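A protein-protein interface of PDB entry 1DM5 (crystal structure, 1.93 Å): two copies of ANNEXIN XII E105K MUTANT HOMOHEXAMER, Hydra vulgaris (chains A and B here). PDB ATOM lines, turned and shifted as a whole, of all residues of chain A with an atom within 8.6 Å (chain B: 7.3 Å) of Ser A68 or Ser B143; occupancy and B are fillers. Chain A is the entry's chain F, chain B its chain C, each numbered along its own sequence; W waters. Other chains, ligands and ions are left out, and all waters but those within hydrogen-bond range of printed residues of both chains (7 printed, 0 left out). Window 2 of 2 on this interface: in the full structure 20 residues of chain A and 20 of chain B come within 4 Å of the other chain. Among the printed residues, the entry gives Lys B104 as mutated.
Of the 16 printed residues of chain A, 5 touch a printed residue of chain B.
No position is printed for both chains. Of the 9 pairs that touch across the chains among the printed residues, none has its exchanged pair printed and touching as well.
Water W1 lies within hydrogen-bond range of the side-chain carboxylate of Asp B229 (2.5 Å) and the side-chain hydroxyl of Ser A68 (2.7 Å). Water W2 lies within hydrogen-bond range of the side-chain hydroxyl (OG) of Ser B143 and the backbone carbonyl oxygen (O) of Asp A64. Water W5 lies within hydrogen-bond range of O of Glu B141 (2.8 Å) and O of Lys A67 (3.0 Å). Water W6 lies within hydrogen-bond range of OG of Ser A68 (3.0 Å) and O of Ser B143 (3.4 Å). Water W4 lies within hydrogen-bond range of OD1 of Asp A64 (3.1 Å), N of Thr B142 (3.2 Å) and O of Ser B140 (3.5 Å). Water W7 lies within hydrogen-bond range of O of Thr B102 (3.2 Å) and OE1 of Glu A75 (3.4 Å).
Asp A64 touches Ser B140. Thr B102 touches Lys A67 (OG1 to CD, 3.7 Å). Ser A68 touches Ser B143 (CB to OG, 3.8 Å).
The side-chain carboxylate (OE2) of Glu A75 sits at hydrogen-bond distance from the backbone NH (N) of Thr B102, 3.0 Å away. NZ of Lys B104 sits at hydrogen-bond distance from O of Lys A67 (2.8 Å). The side-chain amino group (NZ) of Lys B104 sits at hydrogen-bond distance from the backbone carbonyl oxygen (O) of Ser A68 (3.2 Å). The side-chain amino group (NZ) of Lys B104 is in hydrogen-bond range of the backbone carbonyl oxygen (O) of Leu A70 (2.6 Å). The side-chain carboxylate of Glu B141 lies within salt-bridge range of the side-chain amino group of Lys A67, 2.8 Å away. The side-chain carboxylate (OD1) of Asp B229 lies close to the backbone carbonyl oxygen (O) of Ser A68 (3.3 Å).
Glu A63 touches none of the printed residues of chain B. Printed residues of chain B within 4 Å of Lys A67: Thr B102 (3.7 Å), Lys B104 (2.8 Å) and Glu B141 (2.8 Å). Ser A68 touches three residues of chain B. Of the printed residues of chain B, Glu A75 touches Thr B102. Of the printed residues of chain A, Glu B141 touches Lys A67 (2.8 Å). Printed residues of chain A within 4 Å of Ser B143: Ser A68 (3.8 Å). No residue of chain A comes within 4 Å of Gly B144. Arg B148 touches none of the printed residues of chain A. The nearest residue of chain B that does not touch Ser A68 is Glu B141 (5.9 Å). The nearest residue of chain A that does not touch Ser B143 is Asp A64 (4.3 Å).
The backbone carbonyl oxygen (O) of Glu B141 sits at hydrogen-bond distance from the side-chain hydroxyl (OG1) of Thr B102. OD1 of Asp B229 lies within salt-bridge range of NZ of Lys B104. The side-chain carboxylate of Asp A64 lies within salt-bridge range of the side-chain amino group of Lys A67. The side-chain hydroxyl of Ser A68 sits at hydrogen-bond distance from the side-chain carboxylate of Glu A69 (2.8 Å).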
ATOM      1  N   MET A  25     -36.165  16.855  22.894  1.00  0.00           N
ATOM      2  CA  MET A  25     -34.708  16.894  23.057  1.00  0.00           C
ATOM      3  C   MET A  25     -33.976  17.577  21.919  1.00  0.00           C
ATOM      4  O   MET A  25     -32.896  18.133  22.133  1.00  0.00           O
ATOM      5  CB  MET A  25     -34.187  15.456  23.202  1.00  0.00           C
ATOM      6  CG  MET A  25     -34.791  14.782  24.431  1.00  0.00           C
ATOM      7  SD  MET A  25     -34.084  13.145  24.721  1.00  0.00           S
ATOM      8  CE  MET A  25     -34.801  12.245  23.344  1.00  0.00           C
ATOM      9  N   THR A  30     -34.067  21.597  26.607  1.00  0.00           N
ATOM     10  CA  THR A  30     -34.650  20.266  26.794  1.00  0.00           C
ATOM     11  C   THR A  30     -36.015  20.447  27.439  1.00  0.00           C
ATOM     12  O   THR A  30     -36.115  21.167  28.430  1.00  0.00           O
ATOM     13  CB  THR A  30     -33.789  19.367  27.695  1.00  0.00           C
ATOM     14  OG1 THR A  30     -32.469  19.272  27.140  1.00  0.00           O
ATOM     15  CG2 THR A  30     -34.377  17.965  27.752  1.00  0.00           C
ATOM     16  N   LYS A  60     -30.677   5.455  17.465  1.00  0.00           N
ATOM     17  CA  LYS A  60     -30.097   5.671  18.783  1.00  0.00           C
ATOM     18  C   LYS A  60     -31.098   5.205  19.847  1.00  0.00           C
ATOM     19  O   LYS A  60     -32.291   5.502  19.701  1.00  0.00           O
ATOM     20  CB  LYS A  60     -29.837   7.151  19.080  1.00  0.00           C
ATOM     21  CG  LYS A  60     -28.776   7.823  18.228  1.00  0.00           C
ATOM     22  CD  LYS A  60     -28.909   9.334  18.383  1.00  0.00           C
ATOM     23  CE  LYS A  60     -27.578  10.030  18.173  1.00  0.00           C
ATOM     24  NZ  LYS A  60     -27.739  11.506  18.057  1.00  0.00           N
ATOM     25  N   HIS A  61     -30.617   4.550  20.899  1.00  0.00           N
ATOM     26  CA  HIS A  61     -31.566   4.094  21.923  1.00  0.00           C
ATOM     27  C   HIS A  61     -32.006   5.257  22.802  1.00  0.00           C
ATOM     28  O   HIS A  61     -31.198   6.135  23.125  1.00  0.00           O
ATOM     29  CB  HIS A  61     -30.993   2.961  22.778  1.00  0.00           C
ATOM     30  CG  HIS A  61     -30.743   1.692  22.017  1.00  0.00           C
ATOM     31  ND1 HIS A  61     -31.600   0.620  22.049  1.00  0.00           N
ATOM     32  CD2 HIS A  61     -29.743   1.325  21.184  1.00  0.00           C
ATOM     33  CE1 HIS A  61     -31.132  -0.352  21.290  1.00  0.00           C
ATOM     34  NE2 HIS A  61     -29.991   0.054  20.744  1.00  0.00           N
ATOM     35  N   LEU A  62     -33.273   5.228  23.207  1.00  0.00           N
ATOM     36  CA  LEU A  62     -33.856   6.248  24.064  1.00  0.00           C
ATOM     37  C   LEU A  62     -33.082   6.414  25.369  1.00  0.00           C
ATOM     38  O   LEU A  62     -32.852   7.525  25.850  1.00  0.00           O
ATOM     39  CB  LEU A  62     -35.306   5.875  24.372  1.00  0.00           C
ATOM     40  CG  LEU A  62     -36.343   6.989  24.397  1.00  0.00           C
ATOM     41  CD1 LEU A  62     -37.453   6.669  25.387  1.00  0.00           C
ATOM     42  CD2 LEU A  62     -35.704   8.328  24.716  1.00  0.00           C
ATOM     43  N   GLU A  63     -32.689   5.302  25.982  1.00  0.00           N
ATOM     44  CA  GLU A  63     -31.896   5.381  27.208  1.00  0.00           C
ATOM     45  C   GLU A  63     -30.646   6.226  26.987  1.00  0.00           C
ATOM     46  O   GLU A  63     -30.285   7.025  27.854  1.00  0.00           O
ATOM     47  CB  GLU A  63     -31.460   3.989  27.673  1.00  0.00           C
ATOM     48  CG  GLU A  63     -32.619   3.071  27.986  1.00  0.00           C
ATOM     49  CD  GLU A  63     -32.960   2.144  26.837  1.00  0.00           C
ATOM     50  OE1 GLU A  63     -32.858   2.566  25.673  1.00  0.00           O
ATOM     51  OE2 GLU A  63     -33.360   0.991  27.109  1.00  0.00           O
ATOM     52  N   ASP A  64     -29.983   6.020  25.849  1.00  0.00           N
ATOM     53  CA  ASP A  64     -28.748   6.787  25.627  1.00  0.00           C
ATOM     54  C   ASP A  64     -29.007   8.283  25.474  1.00  0.00           C
ATOM     55  O   ASP A  64     -28.311   9.121  26.045  1.00  0.00           O
ATOM     56  CB  ASP A  64     -28.005   6.243  24.413  1.00  0.00           C
ATOM     57  CG  ASP A  64     -27.527   4.822  24.654  1.00  0.00           C
ATOM     58  OD1 ASP A  64     -27.230   4.492  25.820  1.00  0.00           O
ATOM     59  OD2 ASP A  64     -27.532   4.056  23.666  1.00  0.00           O
ATOM     60  N   GLU A  65     -30.054   8.651  24.747  1.00  0.00           N
ATOM     61  CA  GLU A  65     -30.481  10.039  24.676  1.00  0.00           C
ATOM     62  C   GLU A  65     -30.655  10.651  26.060  1.00  0.00           C
ATOM     63  O   GLU A  65     -30.194  11.765  26.314  1.00  0.00           O
ATOM     64  CB  GLU A  65     -31.805  10.158  23.910  1.00  0.00           C
ATOM     65  CG  GLU A  65     -31.796   9.601  22.506  1.00  0.00           C
ATOM     66  CD  GLU A  65     -31.052  10.447  21.492  1.00  0.00           C
ATOM     67  OE1 GLU A  65     -29.860  10.736  21.723  1.00  0.00           O
ATOM     68  OE2 GLU A  65     -31.626  10.752  20.423  1.00  0.00           O
ATOM     69  N   LEU A  66     -31.340   9.936  26.951  1.00  0.00           N
ATOM     70  CA  LEU A  66     -31.624  10.472  28.276  1.00  0.00           C
ATOM     71  C   LEU A  66     -30.376  10.526  29.155  1.00  0.00           C
ATOM     72  O   LEU A  66     -30.292  11.392  30.028  1.00  0.00           O
ATOM     73  CB  LEU A  66     -32.702   9.640  28.982  1.00  0.00           C
ATOM     74  CG  LEU A  66     -34.095   9.711  28.338  1.00  0.00           C
ATOM     75  CD1 LEU A  66     -35.128   9.047  29.237  1.00  0.00           C
ATOM     76  CD2 LEU A  66     -34.443  11.159  28.015  1.00  0.00           C
ATOM     77  N   LYS A  67     -29.456   9.595  28.942  1.00  0.00           N
ATOM     78  CA  LYS A  67     -28.209   9.537  29.694  1.00  0.00           C
ATOM     79  C   LYS A  67     -27.375  10.791  29.437  1.00  0.00           C
ATOM     80  O   LYS A  67     -26.659  11.269  30.311  1.00  0.00           O
ATOM     81  CB  LYS A  67     -27.410   8.299  29.285  1.00  0.00           C
ATOM     82  CG  LYS A  67     -27.846   7.055  30.059  1.00  0.00           C
ATOM     83  CD  LYS A  67     -26.984   5.862  29.659  1.00  0.00           C
ATOM     84  CE  LYS A  67     -27.674   4.548  30.012  1.00  0.00           C
ATOM     85  NZ  LYS A  67     -27.215   3.458  29.092  1.00  0.00           N
ATOM     86  N   SER A  68     -27.533  11.333  28.234  1.00  0.00           N
ATOM     87  CA  SER A  68     -26.834  12.554  27.852  1.00  0.00           C
ATOM     88  C   SER A  68     -27.647  13.790  28.209  1.00  0.00           C
ATOM     89  O   SER A  68     -27.139  14.780  28.729  1.00  0.00           O
ATOM     90  CB  SER A  68     -26.552  12.554  26.344  1.00  0.00           C
ATOM     91  OG  SER A  68     -26.163  13.856  25.920  1.00  0.00           O
ATOM     92  N   GLU A  69     -28.939  13.758  27.890  1.00  0.00           N
ATOM     93  CA  GLU A  69     -29.733  14.974  28.014  1.00  0.00           C
ATOM     94  C   GLU A  69     -30.192  15.250  29.428  1.00  0.00           C
ATOM     95  O   GLU A  69     -30.377  16.415  29.799  1.00  0.00           O
ATOM     96  CB  GLU A  69     -30.894  14.931  27.016  1.00  0.00           C
ATOM     97  CG  GLU A  69     -30.460  15.052  25.559  1.00  0.00           C
ATOM     98  CD  GLU A  69     -29.352  16.065  25.343  1.00  0.00           C
ATOM     99  OE1 GLU A  69     -28.160  15.690  25.415  1.00  0.00           O
ATOM    100  OE2 GLU A  69     -29.615  17.262  25.126  1.00  0.00           O
ATOM    101  N   LEU A  70     -30.393  14.242  30.271  1.00  0.00           N
ATOM    102  CA  LEU A  70     -30.840  14.501  31.637  1.00  0.00           C
ATOM    103  C   LEU A  70     -29.701  14.384  32.643  1.00  0.00           C
ATOM    104  O   LEU A  70     -28.630  13.883  32.327  1.00  0.00           O
ATOM    105  CB  LEU A  70     -31.967  13.534  32.031  1.00  0.00           C
ATOM    106  CG  LEU A  70     -33.162  13.550  31.068  1.00  0.00           C
ATOM    107  CD1 LEU A  70     -34.298  12.673  31.553  1.00  0.00           C
ATOM    108  CD2 LEU A  70     -33.641  14.989  30.885  1.00  0.00           C
ATOM    109  N   SER A  71     -29.957  14.795  33.880  1.00  0.00           N
ATOM    110  CA  SER A  71     -28.951  14.688  34.928  1.00  0.00           C
ATOM    111  C   SER A  71     -29.574  14.372  36.290  1.00  0.00           C
ATOM    112  O   SER A  71     -30.775  14.516  36.497  1.00  0.00           O
ATOM    113  CB  SER A  71     -28.142  15.988  35.014  1.00  0.00           C
ATOM    114  OG  SER A  71     -28.677  16.838  36.024  1.00  0.00           O
ATOM    115  N   GLU A  75     -32.587  12.084  35.889  1.00  0.00           N
ATOM    116  CA  GLU A  75     -32.162  11.088  34.914  1.00  0.00           C
ATOM    117  C   GLU A  75     -32.355   9.677  35.456  1.00  0.00           C
ATOM    118  O   GLU A  75     -32.718   8.742  34.754  1.00  0.00           O
ATOM    119  CB  GLU A  75     -30.673  11.302  34.606  1.00  0.00           C
ATOM    120  CG  GLU A  75     -30.102  10.358  33.556  1.00  0.00           C
ATOM    121  CD  GLU A  75     -28.628  10.061  33.749  1.00  0.00           C
ATOM    122  OE1 GLU A  75     -27.985  10.713  34.601  1.00  0.00           O
ATOM    123  OE2 GLU A  75     -28.110   9.140  33.081  1.00  0.00           O
ATOM    124  N   LEU A  79     -34.794   6.977  33.638  1.00  0.00           N
ATOM    125  CA  LEU A  79     -34.221   5.707  33.193  1.00  0.00           C
ATOM    126  C   LEU A  79     -34.849   4.497  33.877  1.00  0.00           C
ATOM    127  O   LEU A  79     -34.944   3.391  33.326  1.00  0.00           O
ATOM    128  CB  LEU A  79     -32.722   5.753  33.518  1.00  0.00           C
ATOM    129  CG  LEU A  79     -31.728   6.034  32.399  1.00  0.00           C
ATOM    130  CD1 LEU A  79     -32.359   6.490  31.096  1.00  0.00           C
ATOM    131  CD2 LEU A  79     -30.670   7.023  32.865  1.00  0.00           C
ATOM    132  N   THR B 102     -26.039   7.539  34.638  1.00  0.00           N
ATOM    133  CA  THR B 102     -24.623   7.887  34.532  1.00  0.00           C
ATOM    134  C   THR B 102     -24.289   9.040  35.475  1.00  0.00           C
ATOM    135  O   THR B 102     -24.981  10.064  35.438  1.00  0.00           O
ATOM    136  CB  THR B 102     -24.294   8.273  33.076  1.00  0.00           C
ATOM    137  OG1 THR B 102     -24.545   7.191  32.169  1.00  0.00           O
ATOM    138  CG2 THR B 102     -22.822   8.609  32.891  1.00  0.00           C
ATOM    139  N   LYS B 104     -22.224  11.727  35.487  1.00  0.00           N
ATOM    140  CA  LYS B 104     -21.322  12.437  34.592  1.00  0.00           C
ATOM    141  C   LYS B 104     -20.364  13.360  35.303  1.00  0.00           C
ATOM    142  O   LYS B 104     -19.224  13.476  34.849  1.00  0.00           O
ATOM    143  CB  LYS B 104     -22.142  13.122  33.491  1.00  0.00           C
ATOM    144  CG  LYS B 104     -22.950  12.038  32.767  1.00  0.00           C
ATOM    145  CD  LYS B 104     -23.990  12.632  31.842  1.00  0.00           C
ATOM    146  CE  LYS B 104     -25.266  13.017  32.577  1.00  0.00           C
ATOM    147  NZ  LYS B 104     -26.159  13.741  31.615  1.00  0.00           N
ATOM    148  N   ILE B 138     -17.120   3.469  28.525  1.00  0.00           N
ATOM    149  CA  ILE B 138     -17.376   4.901  28.426  1.00  0.00           C
ATOM    150  C   ILE B 138     -18.268   5.212  27.229  1.00  0.00           C
ATOM    151  O   ILE B 138     -19.255   5.939  27.354  1.00  0.00           O
ATOM    152  CB  ILE B 138     -16.044   5.673  28.332  1.00  0.00           C
ATOM    153  CG1 ILE B 138     -15.296   5.753  29.671  1.00  0.00           C
ATOM    154  CG2 ILE B 138     -16.226   7.057  27.743  1.00  0.00           C
ATOM    155  CD1 ILE B 138     -16.117   6.456  30.735  1.00  0.00           C
ATOM    156  N   ILE B 139     -17.933   4.659  26.073  1.00  0.00           N
ATOM    157  CA  ILE B 139     -18.681   4.893  24.837  1.00  0.00           C
ATOM    158  C   ILE B 139     -20.075   4.291  24.876  1.00  0.00           C
ATOM    159  O   ILE B 139     -20.989   4.644  24.126  1.00  0.00           O
ATOM    160  CB  ILE B 139     -17.892   4.302  23.653  1.00  0.00           C
ATOM    161  CG1 ILE B 139     -16.695   5.151  23.222  1.00  0.00           C
ATOM    162  CG2 ILE B 139     -18.816   4.006  22.483  1.00  0.00           C
ATOM    163  CD1 ILE B 139     -15.732   4.409  22.327  1.00  0.00           C
ATOM    164  N   SER B 140     -20.267   3.353  25.799  1.00  0.00           N
ATOM    165  CA  SER B 140     -21.545   2.715  26.046  1.00  0.00           C
ATOM    166  C   SER B 140     -22.469   3.550  26.910  1.00  0.00           C
ATOM    167  O   SER B 140     -23.684   3.323  26.954  1.00  0.00           O
ATOM    168  CB  SER B 140     -21.310   1.384  26.804  1.00  0.00           C
ATOM    169  OG  SER B 140     -20.873   0.433  25.858  1.00  0.00           O
ATOM    170  N   GLU B 141     -21.926   4.488  27.690  1.00  0.00           N
ATOM    171  CA  GLU B 141     -22.781   5.226  28.608  1.00  0.00           C
ATOM    172  C   GLU B 141     -22.708   6.730  28.393  1.00  0.00           C
ATOM    173  O   GLU B 141     -23.218   7.503  29.206  1.00  0.00           O
ATOM    174  CB  GLU B 141     -22.405   4.913  30.063  1.00  0.00           C
ATOM    175  CG  GLU B 141     -22.422   3.415  30.354  1.00  0.00           C
ATOM    176  CD  GLU B 141     -23.829   2.857  30.283  1.00  0.00           C
ATOM    177  OE1 GLU B 141     -23.956   1.647  30.013  1.00  0.00           O
ATOM    178  OE2 GLU B 141     -24.798   3.609  30.494  1.00  0.00           O
ATOM    179  N   THR B 142     -22.057   7.142  27.313  1.00  0.00           N
ATOM    180  CA  THR B 142     -21.981   8.557  26.964  1.00  0.00           C
ATOM    181  C   THR B 142     -22.132   8.680  25.450  1.00  0.00           C
ATOM    182  O   THR B 142     -22.059   7.674  24.752  1.00  0.00           O
ATOM    183  CB  THR B 142     -20.661   9.242  27.357  1.00  0.00           C
ATOM    184  OG1 THR B 142     -19.577   8.545  26.729  1.00  0.00           O
ATOM    185  CG2 THR B 142     -20.408   9.209  28.853  1.00  0.00           C
ATOM    186  N   SER B 143     -22.324   9.899  24.947  1.00  0.00           N
ATOM    187  CA  SER B 143     -22.462  10.049  23.501  1.00  0.00           C
ATOM    188  C   SER B 143     -22.150  11.470  23.056  1.00  0.00           C
ATOM    189  O   SER B 143     -21.940  12.338  23.899  1.00  0.00           O
ATOM    190  CB  SER B 143     -23.864   9.650  23.024  1.00  0.00           C
ATOM    191  OG  SER B 143     -24.875  10.316  23.759  1.00  0.00           O
ATOM    192  N   GLY B 144     -22.142  11.689  21.749  1.00  0.00           N
ATOM    193  CA  GLY B 144     -21.912  12.995  21.164  1.00  0.00           C
ATOM    194  C   GLY B 144     -20.592  13.623  21.555  1.00  0.00           C
ATOM    195  O   GLY B 144     -19.551  12.991  21.747  1.00  0.00           O
ATOM    196  N   ASN B 145     -20.603  14.943  21.717  1.00  0.00           N
ATOM    197  CA  ASN B 145     -19.375  15.674  21.997  1.00  0.00           C
ATOM    198  C   ASN B 145     -18.811  15.300  23.355  1.00  0.00           C
ATOM    199  O   ASN B 145     -17.593  15.302  23.558  1.00  0.00           O
ATOM    200  CB  ASN B 145     -19.601  17.185  21.900  1.00  0.00           C
ATOM    201  CG  ASN B 145     -19.805  17.659  20.474  1.00  0.00           C
ATOM    202  OD1 ASN B 145     -19.452  16.982  19.504  1.00  0.00           O
ATOM    203  ND2 ASN B 145     -20.352  18.867  20.335  1.00  0.00           N
ATOM    204  N   PHE B 146     -19.692  15.018  24.310  1.00  0.00           N
ATOM    205  CA  PHE B 146     -19.199  14.670  25.640  1.00  0.00           C
ATOM    206  C   PHE B 146     -18.421  13.362  25.579  1.00  0.00           C
ATOM    207  O   PHE B 146     -17.301  13.301  26.078  1.00  0.00           O
ATOM    208  CB  PHE B 146     -20.348  14.665  26.638  1.00  0.00           C
ATOM    209  CG  PHE B 146     -19.918  14.341  28.061  1.00  0.00           C
ATOM    210  CD1 PHE B 146     -18.969  15.122  28.689  1.00  0.00           C
ATOM    211  CD2 PHE B 146     -20.448  13.255  28.731  1.00  0.00           C
ATOM    212  CE1 PHE B 146     -18.569  14.838  29.979  1.00  0.00           C
ATOM    213  CE2 PHE B 146     -20.085  12.982  30.040  1.00  0.00           C
ATOM    214  CZ  PHE B 146     -19.134  13.776  30.662  1.00  0.00           C
ATOM    215  N   GLN B 147     -18.922  12.337  24.895  1.00  0.00           N
ATOM    216  CA  GLN B 147     -18.205  11.089  24.693  1.00  0.00           C
ATOM    217  C   GLN B 147     -16.817  11.312  24.095  1.00  0.00           C
ATOM    218  O   GLN B 147     -15.806  10.786  24.564  1.00  0.00           O
ATOM    219  CB  GLN B 147     -18.975  10.169  23.730  1.00  0.00           C
ATOM    220  CG  GLN B 147     -18.187   8.932  23.326  1.00  0.00           C
ATOM    221  CD  GLN B 147     -18.815   8.151  22.185  1.00  0.00           C
ATOM    222  OE1 GLN B 147     -18.242   7.945  21.116  1.00  0.00           O
ATOM    223  NE2 GLN B 147     -20.014   7.637  22.406  1.00  0.00           N
ATOM    224  N   ARG B 148     -16.790  12.084  23.015  1.00  0.00           N
ATOM    225  CA  ARG B 148     -15.550  12.386  22.302  1.00  0.00           C
ATOM    226  C   ARG B 148     -14.515  13.029  23.215  1.00  0.00           C
ATOM    227  O   ARG B 148     -13.336  12.664  23.180  1.00  0.00           O
ATOM    228  CB  ARG B 148     -15.843  13.282  21.082  1.00  0.00           C
ATOM    229  CG  ARG B 148     -16.329  12.473  19.877  1.00  0.00           C
ATOM    230  CD  ARG B 148     -16.993  13.390  18.839  1.00  0.00           C
ATOM    231  NE  ARG B 148     -18.177  12.707  18.354  1.00  0.00           N
ATOM    232  CZ  ARG B 148     -19.427  13.060  18.199  1.00  0.00           C
ATOM    233  NH1 ARG B 148     -19.885  14.288  18.450  1.00  0.00           N
ATOM    234  NH2 ARG B 148     -20.271  12.147  17.731  1.00  0.00           N
ATOM    235  N   LEU B 149     -14.931  13.974  24.059  1.00  0.00           N
ATOM    236  CA  LEU B 149     -14.004  14.580  25.013  1.00  0.00           C
ATOM    237  C   LEU B 149     -13.445  13.508  25.938  1.00  0.00           C
ATOM    238  O   LEU B 149     -12.250  13.515  26.212  1.00  0.00           O
ATOM    239  CB  LEU B 149     -14.676  15.659  25.872  1.00  0.00           C
ATOM    240  CG  LEU B 149     -13.752  16.296  26.924  1.00  0.00           C
ATOM    241  CD1 LEU B 149     -12.596  17.003  26.240  1.00  0.00           C
ATOM    242  CD2 LEU B 149     -14.481  17.247  27.847  1.00  0.00           C
ATOM    243  N   LEU B 150     -14.301  12.609  26.421  1.00  0.00           N
ATOM    244  CA  LEU B 150     -13.834  11.543  27.317  1.00  0.00           C
ATOM    245  C   LEU B 150     -12.913  10.586  26.595  1.00  0.00           C
ATOM    246  O   LEU B 150     -11.841  10.172  27.067  1.00  0.00           O
ATOM    247  CB  LEU B 150     -15.031  10.845  27.949  1.00  0.00           C
ATOM    248  CG  LEU B 150     -15.922  11.651  28.894  1.00  0.00           C
ATOM    249  CD1 LEU B 150     -16.853  10.716  29.667  1.00  0.00           C
ATOM    250  CD2 LEU B 150     -15.098  12.471  29.874  1.00  0.00           C
ATOM    251  N   GLY B 228     -24.528  21.813  29.386  1.00  0.00           N
ATOM    252  CA  GLY B 228     -24.538  20.426  29.802  1.00  0.00           C
ATOM    253  C   GLY B 228     -23.170  19.820  30.024  1.00  0.00           C
ATOM    254  O   GLY B 228     -22.226  20.501  30.417  1.00  0.00           O
ATOM    255  N   ASP B 229     -23.066  18.511  29.807  1.00  0.00           N
ATOM    256  CA  ASP B 229     -21.851  17.762  30.090  1.00  0.00           C
ATOM    257  C   ASP B 229     -20.652  18.305  29.342  1.00  0.00           C
ATOM    258  O   ASP B 229     -19.581  18.451  29.939  1.00  0.00           O
ATOM    259  CB  ASP B 229     -22.042  16.278  29.741  1.00  0.00           C
ATOM    260  CG  ASP B 229     -23.264  15.706  30.450  1.00  0.00           C
ATOM    261  OD1 ASP B 229     -24.047  14.985  29.795  1.00  0.00           O
ATOM    262  OD2 ASP B 229     -23.430  16.013  31.652  1.00  0.00           O
HETATM  263  O   HOH W   1     -23.972  14.508  27.373  1.00  0.00           O
HETATM  264  O   HOH W   2     -25.416   8.843  26.070  1.00  0.00           O
HETATM  265  O   HOH W   3     -27.353   9.310  22.294  1.00  0.00           O
HETATM  266  O   HOH W   4     -24.846   6.448  25.985  1.00  0.00           O
HETATM  267  O   HOH W   5     -23.950  10.198  29.676  1.00  0.00           O
HETATM  268  O   HOH W   6     -24.746  14.239  23.326  1.00  0.00           O
HETATM  269  O   HOH W   7     -26.014  12.936  36.251  1.00  0.00           O
